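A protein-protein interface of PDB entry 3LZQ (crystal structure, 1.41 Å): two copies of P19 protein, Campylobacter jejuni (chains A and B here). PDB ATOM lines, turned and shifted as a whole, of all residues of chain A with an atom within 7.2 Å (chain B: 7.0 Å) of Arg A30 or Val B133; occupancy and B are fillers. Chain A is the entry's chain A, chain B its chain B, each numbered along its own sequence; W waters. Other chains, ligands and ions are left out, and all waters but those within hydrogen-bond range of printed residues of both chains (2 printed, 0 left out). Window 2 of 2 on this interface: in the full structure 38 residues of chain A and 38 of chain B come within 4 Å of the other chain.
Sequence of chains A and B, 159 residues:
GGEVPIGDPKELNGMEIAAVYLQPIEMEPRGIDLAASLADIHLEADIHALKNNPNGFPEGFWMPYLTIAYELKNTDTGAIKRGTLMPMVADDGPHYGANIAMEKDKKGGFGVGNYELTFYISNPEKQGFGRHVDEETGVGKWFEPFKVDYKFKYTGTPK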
ATOM      1  N   ILE A  25     -15.373  13.780  -7.915  1.00  0.00           N
ATOM      2  CA  ILE A  25     -13.921  14.062  -7.781  1.00  0.00           C
ATOM      3  C   ILE A  25     -13.171  12.806  -7.331  1.00  0.00           C
ATOM      4  O   ILE A  25     -13.779  11.802  -7.000  1.00  0.00           O
ATOM      5  CB  ILE A  25     -13.655  15.232  -6.798  1.00  0.00           C
ATOM      6  CG1 ILE A  25     -14.173  14.943  -5.383  1.00  0.00           C
ATOM      7  CG2 ILE A  25     -14.351  16.488  -7.333  1.00  0.00           C
ATOM      8  CD1 ILE A  25     -13.266  13.965  -4.491  1.00  0.00           C
ATOM      9  N   GLU A  26     -11.851  12.831  -7.435  1.00  0.00           N
ATOM     10  CA  GLU A  26     -11.011  11.714  -7.007  1.00  0.00           C
ATOM     11  C   GLU A  26     -10.313  12.108  -5.729  1.00  0.00           C
ATOM     12  O   GLU A  26      -9.572  13.101  -5.714  1.00  0.00           O
ATOM     13  CB  GLU A  26      -9.937  11.412  -8.049  1.00  0.00           C
ATOM     14  CG  GLU A  26     -10.443  11.074  -9.436  1.00  0.00           C
ATOM     15  CD  GLU A  26      -9.317  10.924 -10.463  1.00  0.00           C
ATOM     16  OE1 GLU A  26      -8.208  10.409 -10.140  1.00  0.00           O
ATOM     17  OE2 GLU A  26      -9.553  11.323 -11.620  1.00  0.00           O
ATOM     18  N   MET A  27     -10.569  11.371  -4.646  1.00  0.00           N
ATOM     19  CA  MET A  27     -10.017  11.719  -3.335  1.00  0.00           C
ATOM     20  C   MET A  27      -8.985  10.693  -2.859  1.00  0.00           C
ATOM     21  O   MET A  27      -9.177   9.473  -3.017  1.00  0.00           O
ATOM     22  CB  MET A  27     -11.127  11.828  -2.281  1.00  0.00           C
ATOM     23  CG  MET A  27     -10.663  12.446  -0.939  1.00  0.00           C
ATOM     24  SD  MET A  27     -11.830  12.329   0.429  1.00  0.00           S
ATOM     25  CE  MET A  27     -11.410  10.678   1.043  1.00  0.00           C
ATOM     26  N   GLU A  28      -7.905  11.205  -2.274  1.00  0.00           N
ATOM     27  CA  GLU A  28      -6.973  10.391  -1.468  1.00  0.00           C
ATOM     28  C   GLU A  28      -7.112  10.773   0.013  1.00  0.00           C
ATOM     29  O   GLU A  28      -7.420  11.901   0.327  1.00  0.00           O
ATOM     30  CB  GLU A  28      -5.528  10.584  -1.917  1.00  0.00           C
ATOM     31  CG  GLU A  28      -5.231   9.950  -3.236  1.00  0.00           C
ATOM     32  CD  GLU A  28      -3.775  10.035  -3.623  1.00  0.00           C
ATOM     33  OE1 GLU A  28      -2.917  10.379  -2.772  1.00  0.00           O
ATOM     34  OE2 GLU A  28      -3.480   9.758  -4.799  1.00  0.00           O
ATOM     35  N   PRO A  29      -6.909   9.820   0.932  1.00  0.00           N
ATOM     36  CA  PRO A  29      -6.603   8.420   0.637  1.00  0.00           C
ATOM     37  C   PRO A  29      -7.770   7.682  -0.044  1.00  0.00           C
ATOM     38  O   PRO A  29      -8.921   8.084   0.085  1.00  0.00           O
ATOM     39  CB  PRO A  29      -6.303   7.836   2.015  1.00  0.00           C
ATOM     40  CG  PRO A  29      -7.017   8.681   2.975  1.00  0.00           C
ATOM     41  CD  PRO A  29      -7.120  10.064   2.375  1.00  0.00           C
ATOM     42  N   ARG A  30      -7.458   6.600  -0.754  1.00  0.00           N
ATOM     43  CA  ARG A  30      -8.462   5.869  -1.528  1.00  0.00           C
ATOM     44  C   ARG A  30      -9.206   4.891  -0.624  1.00  0.00           C
ATOM     45  O   ARG A  30      -8.737   4.554   0.457  1.00  0.00           O
ATOM     46  CB  ARG A  30      -7.811   5.081  -2.679  1.00  0.00           C
ATOM     47  CG  ARG A  30      -6.836   5.873  -3.553  1.00  0.00           C
ATOM     48  CD  ARG A  30      -7.522   6.588  -4.722  1.00  0.00           C
ATOM     49  NE  ARG A  30      -6.541   7.319  -5.534  1.00  0.00           N
ATOM     50  CZ  ARG A  30      -6.793   7.967  -6.674  1.00  0.00           C
ATOM     51  NH1 ARG A  30      -8.015   7.996  -7.195  1.00  0.00           N
ATOM     52  NH2 ARG A  30      -5.799   8.594  -7.302  1.00  0.00           N
ATOM     53  N   GLY A  31     -10.366   4.440  -1.083  1.00  0.00           N
ATOM     54  CA  GLY A  31     -11.107   3.373  -0.404  1.00  0.00           C
ATOM     55  C   GLY A  31     -12.036   3.872   0.682  1.00  0.00           C
ATOM     56  O   GLY A  31     -12.569   3.079   1.455  1.00  0.00           O
ATOM     57  N   ILE A  32     -12.241   5.181   0.723  1.00  0.00           N
ATOM     58  CA  ILE A  32     -13.099   5.814   1.719  1.00  0.00           C
ATOM     59  C   ILE A  32     -14.292   6.498   1.031  1.00  0.00           C
ATOM     60  O   ILE A  32     -15.440   6.088   1.210  1.00  0.00           O
ATOM     61  CB  ILE A  32     -12.306   6.836   2.567  1.00  0.00           C
ATOM     62  CG1 ILE A  32     -11.058   6.184   3.165  1.00  0.00           C
ATOM     63  CG2 ILE A  32     -13.181   7.408   3.688  1.00  0.00           C
ATOM     64  CD1 ILE A  32     -11.355   4.915   3.979  1.00  0.00           C
ATOM     65  N   ASP A  33     -14.012   7.535   0.244  1.00  0.00           N
ATOM     66  CA  ASP A  33     -15.041   8.225  -0.543  1.00  0.00           C
ATOM     67  C   ASP A  33     -15.429   7.328  -1.721  1.00  0.00           C
ATOM     68  O   ASP A  33     -14.554   6.696  -2.331  1.00  0.00           O
ATOM     69  CB  ASP A  33     -14.489   9.560  -1.051  1.00  0.00           C
ATOM     70  CG  ASP A  33     -15.575  10.493  -1.608  1.00  0.00           C
ATOM     71  OD1 ASP A  33     -16.632  10.656  -0.980  1.00  0.00           O
ATOM     72  OD2 ASP A  33     -15.320  11.086  -2.676  1.00  0.00           O
ATOM     73  N   ALA A  36     -15.033   7.954  -7.979  1.00  0.00           N
ATOM     74  CA  ALA A  36     -15.574   8.910  -8.976  1.00  0.00           C
ATOM     75  C   ALA A  36     -16.487   8.247 -10.015  1.00  0.00           C
ATOM     76  O   ALA A  36     -17.580   8.756 -10.312  1.00  0.00           O
ATOM     77  CB  ALA A  36     -14.444   9.678  -9.675  1.00  0.00           C
ATOM     78  N   VAL A  89      -9.494  18.684   1.276  1.00  0.00           N
ATOM     79  CA  VAL A  89      -9.055  19.918   0.607  1.00  0.00           C
ATOM     80  C   VAL A  89      -9.056  19.753  -0.931  1.00  0.00           C
ATOM     81  O   VAL A  89      -8.669  18.705  -1.458  1.00  0.00           O
ATOM     82  CB  VAL A  89      -7.685  20.431   1.170  1.00  0.00           C
ATOM     83  CG1 VAL A  89      -6.485  19.540   0.768  1.00  0.00           C
ATOM     84  CG2 VAL A  89      -7.441  21.895   0.721  1.00  0.00           C
ATOM     85  N   ALA A  90      -9.472  20.819  -1.617  1.00  0.00           N
ATOM     86  CA  ALA A  90      -9.491  20.936  -3.082  1.00  0.00           C
ATOM     87  C   ALA A  90      -8.824  22.263  -3.411  1.00  0.00           C
ATOM     88  O   ALA A  90      -8.351  22.956  -2.494  1.00  0.00           O
ATOM     89  CB  ALA A  90     -10.947  20.849  -3.649  1.00  0.00           C
ATOM     90  N   GLU B 125      -3.366  13.858   6.362  1.00  0.00           N
ATOM     91  CA  GLU B 125      -3.788  12.545   5.904  1.00  0.00           C
ATOM     92  C   GLU B 125      -3.615  11.496   6.995  1.00  0.00           C
ATOM     93  O   GLU B 125      -4.374  10.524   7.060  1.00  0.00           O
ATOM     94  CB  GLU B 125      -3.004  12.148   4.658  1.00  0.00           C
ATOM     95  CG  GLU B 125      -3.792  11.310   3.702  1.00  0.00           C
ATOM     96  CD  GLU B 125      -2.910  10.592   2.717  1.00  0.00           C
ATOM     97  OE1 GLU B 125      -1.952  11.218   2.220  1.00  0.00           O
ATOM     98  OE2 GLU B 125      -3.178   9.405   2.445  1.00  0.00           O
ATOM     99  N   ARG B 131      -7.783  14.712   0.234  1.00  0.00           N
ATOM    100  CA  ARG B 131      -7.423  15.711  -0.779  1.00  0.00           C
ATOM    101  C   ARG B 131      -7.923  15.278  -2.127  1.00  0.00           C
ATOM    102  O   ARG B 131      -7.842  14.086  -2.486  1.00  0.00           O
ATOM    103  CB  ARG B 131      -5.917  16.055  -0.827  1.00  0.00           C
ATOM    104  CG  ARG B 131      -5.044  15.058  -1.460  1.00  0.00           C
ATOM    105  CD  ARG B 131      -3.617  15.516  -1.472  1.00  0.00           C
ATOM    106  NE  ARG B 131      -2.853  14.409  -2.002  1.00  0.00           N
ATOM    107  CZ  ARG B 131      -2.328  14.325  -3.223  1.00  0.00           C
ATOM    108  NH1 ARG B 131      -2.413  15.331  -4.101  1.00  0.00           N
ATOM    109  NH2 ARG B 131      -1.677  13.230  -3.568  1.00  0.00           N
ATOM    110  N   HIS B 132      -8.434  16.247  -2.889  1.00  0.00           N
ATOM    111  CA  HIS B 132      -8.827  15.991  -4.245  1.00  0.00           C
ATOM    112  C   HIS B 132      -7.532  15.840  -5.037  1.00  0.00           C
ATOM    113  O   HIS B 132      -6.588  16.589  -4.837  1.00  0.00           O
ATOM    114  CB  HIS B 132      -9.675  17.133  -4.828  1.00  0.00           C
ATOM    115  CG  HIS B 132     -11.030  17.303  -4.204  1.00  0.00           C
ATOM    116  ND1 HIS B 132     -12.063  17.937  -4.854  1.00  0.00           N
ATOM    117  CD2 HIS B 132     -11.523  16.880  -3.030  1.00  0.00           C
ATOM    118  CE1 HIS B 132     -13.122  18.004  -4.049  1.00  0.00           C
ATOM    119  NE2 HIS B 132     -12.820  17.308  -2.952  1.00  0.00           N
ATOM    120  N   VAL B 133      -7.530  14.871  -5.939  1.00  0.00           N
ATOM    121  CA  VAL B 133      -6.383  14.585  -6.814  1.00  0.00           C
ATOM    122  C   VAL B 133      -6.715  14.565  -8.327  1.00  0.00           C
ATOM    123  O   VAL B 133      -5.803  14.411  -9.172  1.00  0.00           O
ATOM    124  CB  VAL B 133      -5.654  13.270  -6.420  1.00  0.00           C
ATOM    125  CG1 VAL B 133      -5.199  13.340  -4.960  1.00  0.00           C
ATOM    126  CG2 VAL B 133      -6.541  12.049  -6.668  1.00  0.00           C
ATOM    127  N   ASP B 134      -7.988  14.809  -8.657  1.00  0.00           N
ATOM    128  CA  ASP B 134      -8.417  14.953 -10.048  1.00  0.00           C
ATOM    129  C   ASP B 134      -7.819  16.221 -10.690  1.00  0.00           C
ATOM    130  O   ASP B 134      -7.402  17.185 -10.007  1.00  0.00           O
ATOM    131  CB  ASP B 134      -9.930  14.951 -10.164  1.00  0.00           C
ATOM    132  CG  ASP B 134     -10.562  15.916  -9.218  1.00  0.00           C
ATOM    133  OD1 ASP B 134     -10.570  15.542  -8.023  1.00  0.00           O
ATOM    134  OD2 ASP B 134     -10.954  17.026  -9.654  1.00  0.00           O
ATOM    135  N   GLU B 135      -7.701  16.180 -12.018  1.00  0.00           N
ATOM    136  CA  GLU B 135      -7.087  17.278 -12.748  1.00  0.00           C
ATOM    137  C   GLU B 135      -7.809  18.589 -12.489  1.00  0.00           C
ATOM    138  O   GLU B 135      -7.180  19.637 -12.291  1.00  0.00           O
ATOM    139  CB  GLU B 135      -7.059  16.985 -14.264  1.00  0.00           C
ATOM    140  CG  GLU B 135      -6.407  18.083 -15.099  1.00  0.00           C
ATOM    141  CD  GLU B 135      -6.496  17.843 -16.614  1.00  0.00           C
ATOM    142  OE1 GLU B 135      -6.893  16.732 -17.063  1.00  0.00           O
ATOM    143  OE2 GLU B 135      -6.168  18.790 -17.363  1.00  0.00           O
ATOM    144  N   GLU B 136      -9.134  18.528 -12.492  1.00  0.00           N
ATOM    145  CA  GLU B 136      -9.927  19.736 -12.481  1.00  0.00           C
ATOM    146  C   GLU B 136      -9.855  20.457 -11.125  1.00  0.00           C
ATOM    147  O   GLU B 136      -9.742  21.676 -11.102  1.00  0.00           O
ATOM    148  CB  GLU B 136     -11.379  19.428 -12.834  1.00  0.00           C
ATOM    149  CG  GLU B 136     -12.287  20.687 -12.852  1.00  0.00           C
ATOM    150  CD  GLU B 136     -11.977  21.649 -14.001  1.00  0.00           C
ATOM    151  OE1 GLU B 136     -11.935  21.191 -15.166  1.00  0.00           O
ATOM    152  OE2 GLU B 136     -11.797  22.863 -13.737  1.00  0.00           O
ATOM    153  N   THR B 137      -9.908  19.710 -10.019  1.00  0.00           N
ATOM    154  CA  THR B 137     -10.007  20.321  -8.693  1.00  0.00           C
ATOM    155  C   THR B 137      -8.922  19.919  -7.693  1.00  0.00           C
ATOM    156  O   THR B 137      -8.933  20.369  -6.534  1.00  0.00           O
ATOM    157  CB  THR B 137     -11.376  19.994  -8.063  1.00  0.00           C
ATOM    158  OG1 THR B 137     -11.379  18.620  -7.632  1.00  0.00           O
ATOM    159  CG2 THR B 137     -12.472  20.201  -9.085  1.00  0.00           C
ATOM    160  N   GLY B 138      -7.945  19.138  -8.142  1.00  0.00           N
ATOM    161  CA  GLY B 138      -6.970  18.595  -7.219  1.00  0.00           C
ATOM    162  C   GLY B 138      -5.849  19.556  -6.843  1.00  0.00           C
ATOM    163  O   GLY B 138      -5.667  20.639  -7.428  1.00  0.00           O
ATOM    164  N   VAL B 139      -5.104  19.125  -5.841  1.00  0.00           N
ATOM    165  CA  VAL B 139      -4.033  19.895  -5.225  1.00  0.00           C
ATOM    166  C   VAL B 139      -2.810  18.994  -5.094  1.00  0.00           C
ATOM    167  O   VAL B 139      -2.874  17.797  -5.392  1.00  0.00           O
ATOM    168  CB  VAL B 139      -4.424  20.412  -3.832  1.00  0.00           C
ATOM    169  CG1 VAL B 139      -5.664  21.261  -3.902  1.00  0.00           C
ATOM    170  CG2 VAL B 139      -4.578  19.248  -2.866  1.00  0.00           C
ATOM    171  N   GLY B 140      -1.684  19.590  -4.703  1.00  0.00           N
ATOM    172  CA  GLY B 140      -0.443  18.871  -4.642  1.00  0.00           C
ATOM    173  C   GLY B 140      -0.371  17.901  -3.499  1.00  0.00           C
ATOM    174  O   GLY B 140      -1.211  17.938  -2.560  1.00  0.00           O
HETATM  175  O   HOH W   1      -2.647  12.116  -0.677  1.00  0.00           O
HETATM  176  O   HOH W   2      -5.227  13.933   2.108  1.00  0.00           O
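NH2 of Arg B131 is in salt-bridge range of OE1 of Glu A28.
N of Val B133 is in hydrogen-bond range of O of Glu A26, at 2.7 Å.
O of Val A89 sits at hydrogen-bond distance from N of His B132 (2.9 Å).
N of Glu A26 lies within hydrogen-bond range of OD1 of Asp B134 (3.1 Å).
O of His B132 sits at hydrogen-bond distance from N of Val B139 (3.1 Å).
A ring nitrogen (ND1) of His B132 lies within hydrogen-bond range of the side-chain hydroxyl of Thr B137, at 2.9 Å.
The guanidinium group (NH1) of Arg B131 lies within hydrogen-bond range of the backbone carbonyl oxygen (O) of Val B139.
NH2 of Arg A30 lies within salt-bridge range of OE2 of Glu A28, 3.6 Å away.
The guanidinium group (NH1) of Arg A30 lies within salt-bridge range of the side-chain carboxylate (OE1) of Glu A26 (3.8 Å).
The side-chain hydroxyl (OG1) of Thr B137 lies within hydrogen-bond range of the side-chain carboxylate (OD2) of Asp B134.
Ile A25 touches His B132.
Asp B134 touches Ile A25 (OD1 to CB, 3.3 Å).
OG1 of Thr B137 touches CG2 of Ile A25, at 3.7 Å.
Arg B131 touches Glu A26.
Glu A26 touches His B132.
Arg B131 touches Met A27 (O to CA, 3.3 Å).
Glu A28 touches Val B133.
Pro A29 touches Glu B125.
CG2 of Val B133 touches NH2 of Arg A30, 3.6 Å away.
Ala A90 touches Val B139.
Printed residues of chain B within 4 Å of Pro A29: Glu B125 (3.5 Å).
Arg A30 touches just one residue of chain B: Val B133.
Gly A31 touches none of the printed residues of chain B.
Of the printed residues of chain B, Ala A90 touches His B132, Thr B137 and Val B139.
Printed residues of chain A within 4 Å of Glu B125: Pro A29.
Of the printed residues of chain A, Thr B137 touches Ile A25 (3.7 Å) and Ala A90 (3.5 Å).
Gly B138 touches none of the printed residues of chain A.
The nearest printed residue of chain B that does not touch Ala A90 is Gly B138 (5.3 Å).
Hydrophobic or aromatic side chains of chain A within 4 Å of the printed part of chain B: Ile A25, Met A27, Pro A29, Val A89 and Ala A90.
Along chain A the printed residues that touch a printed residue of chain B span positions 25 to 90.
Among the printed residues, Asp or Glu carboxylates within 4 Å of a Lys or Arg side-chain nitrogen of the other chain: Glu A28 with Arg B131.
No position is printed for both chains.
Of the 17 pairs that touch across the chains among the printed residues, none has its exchanged pair printed and touching as well.
Water W1 lies within hydrogen-bond range of the guanidinium group of Arg B131 (2.7 Å), the side-chain carboxylate of Glu A28 (2.7 Å) and the side-chain carboxylate of Glu B125 (3.1 Å).
Water W2 lies within hydrogen-bond range of N of Arg B131 (3.3 Å) and O of Glu A28 (3.5 Å).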
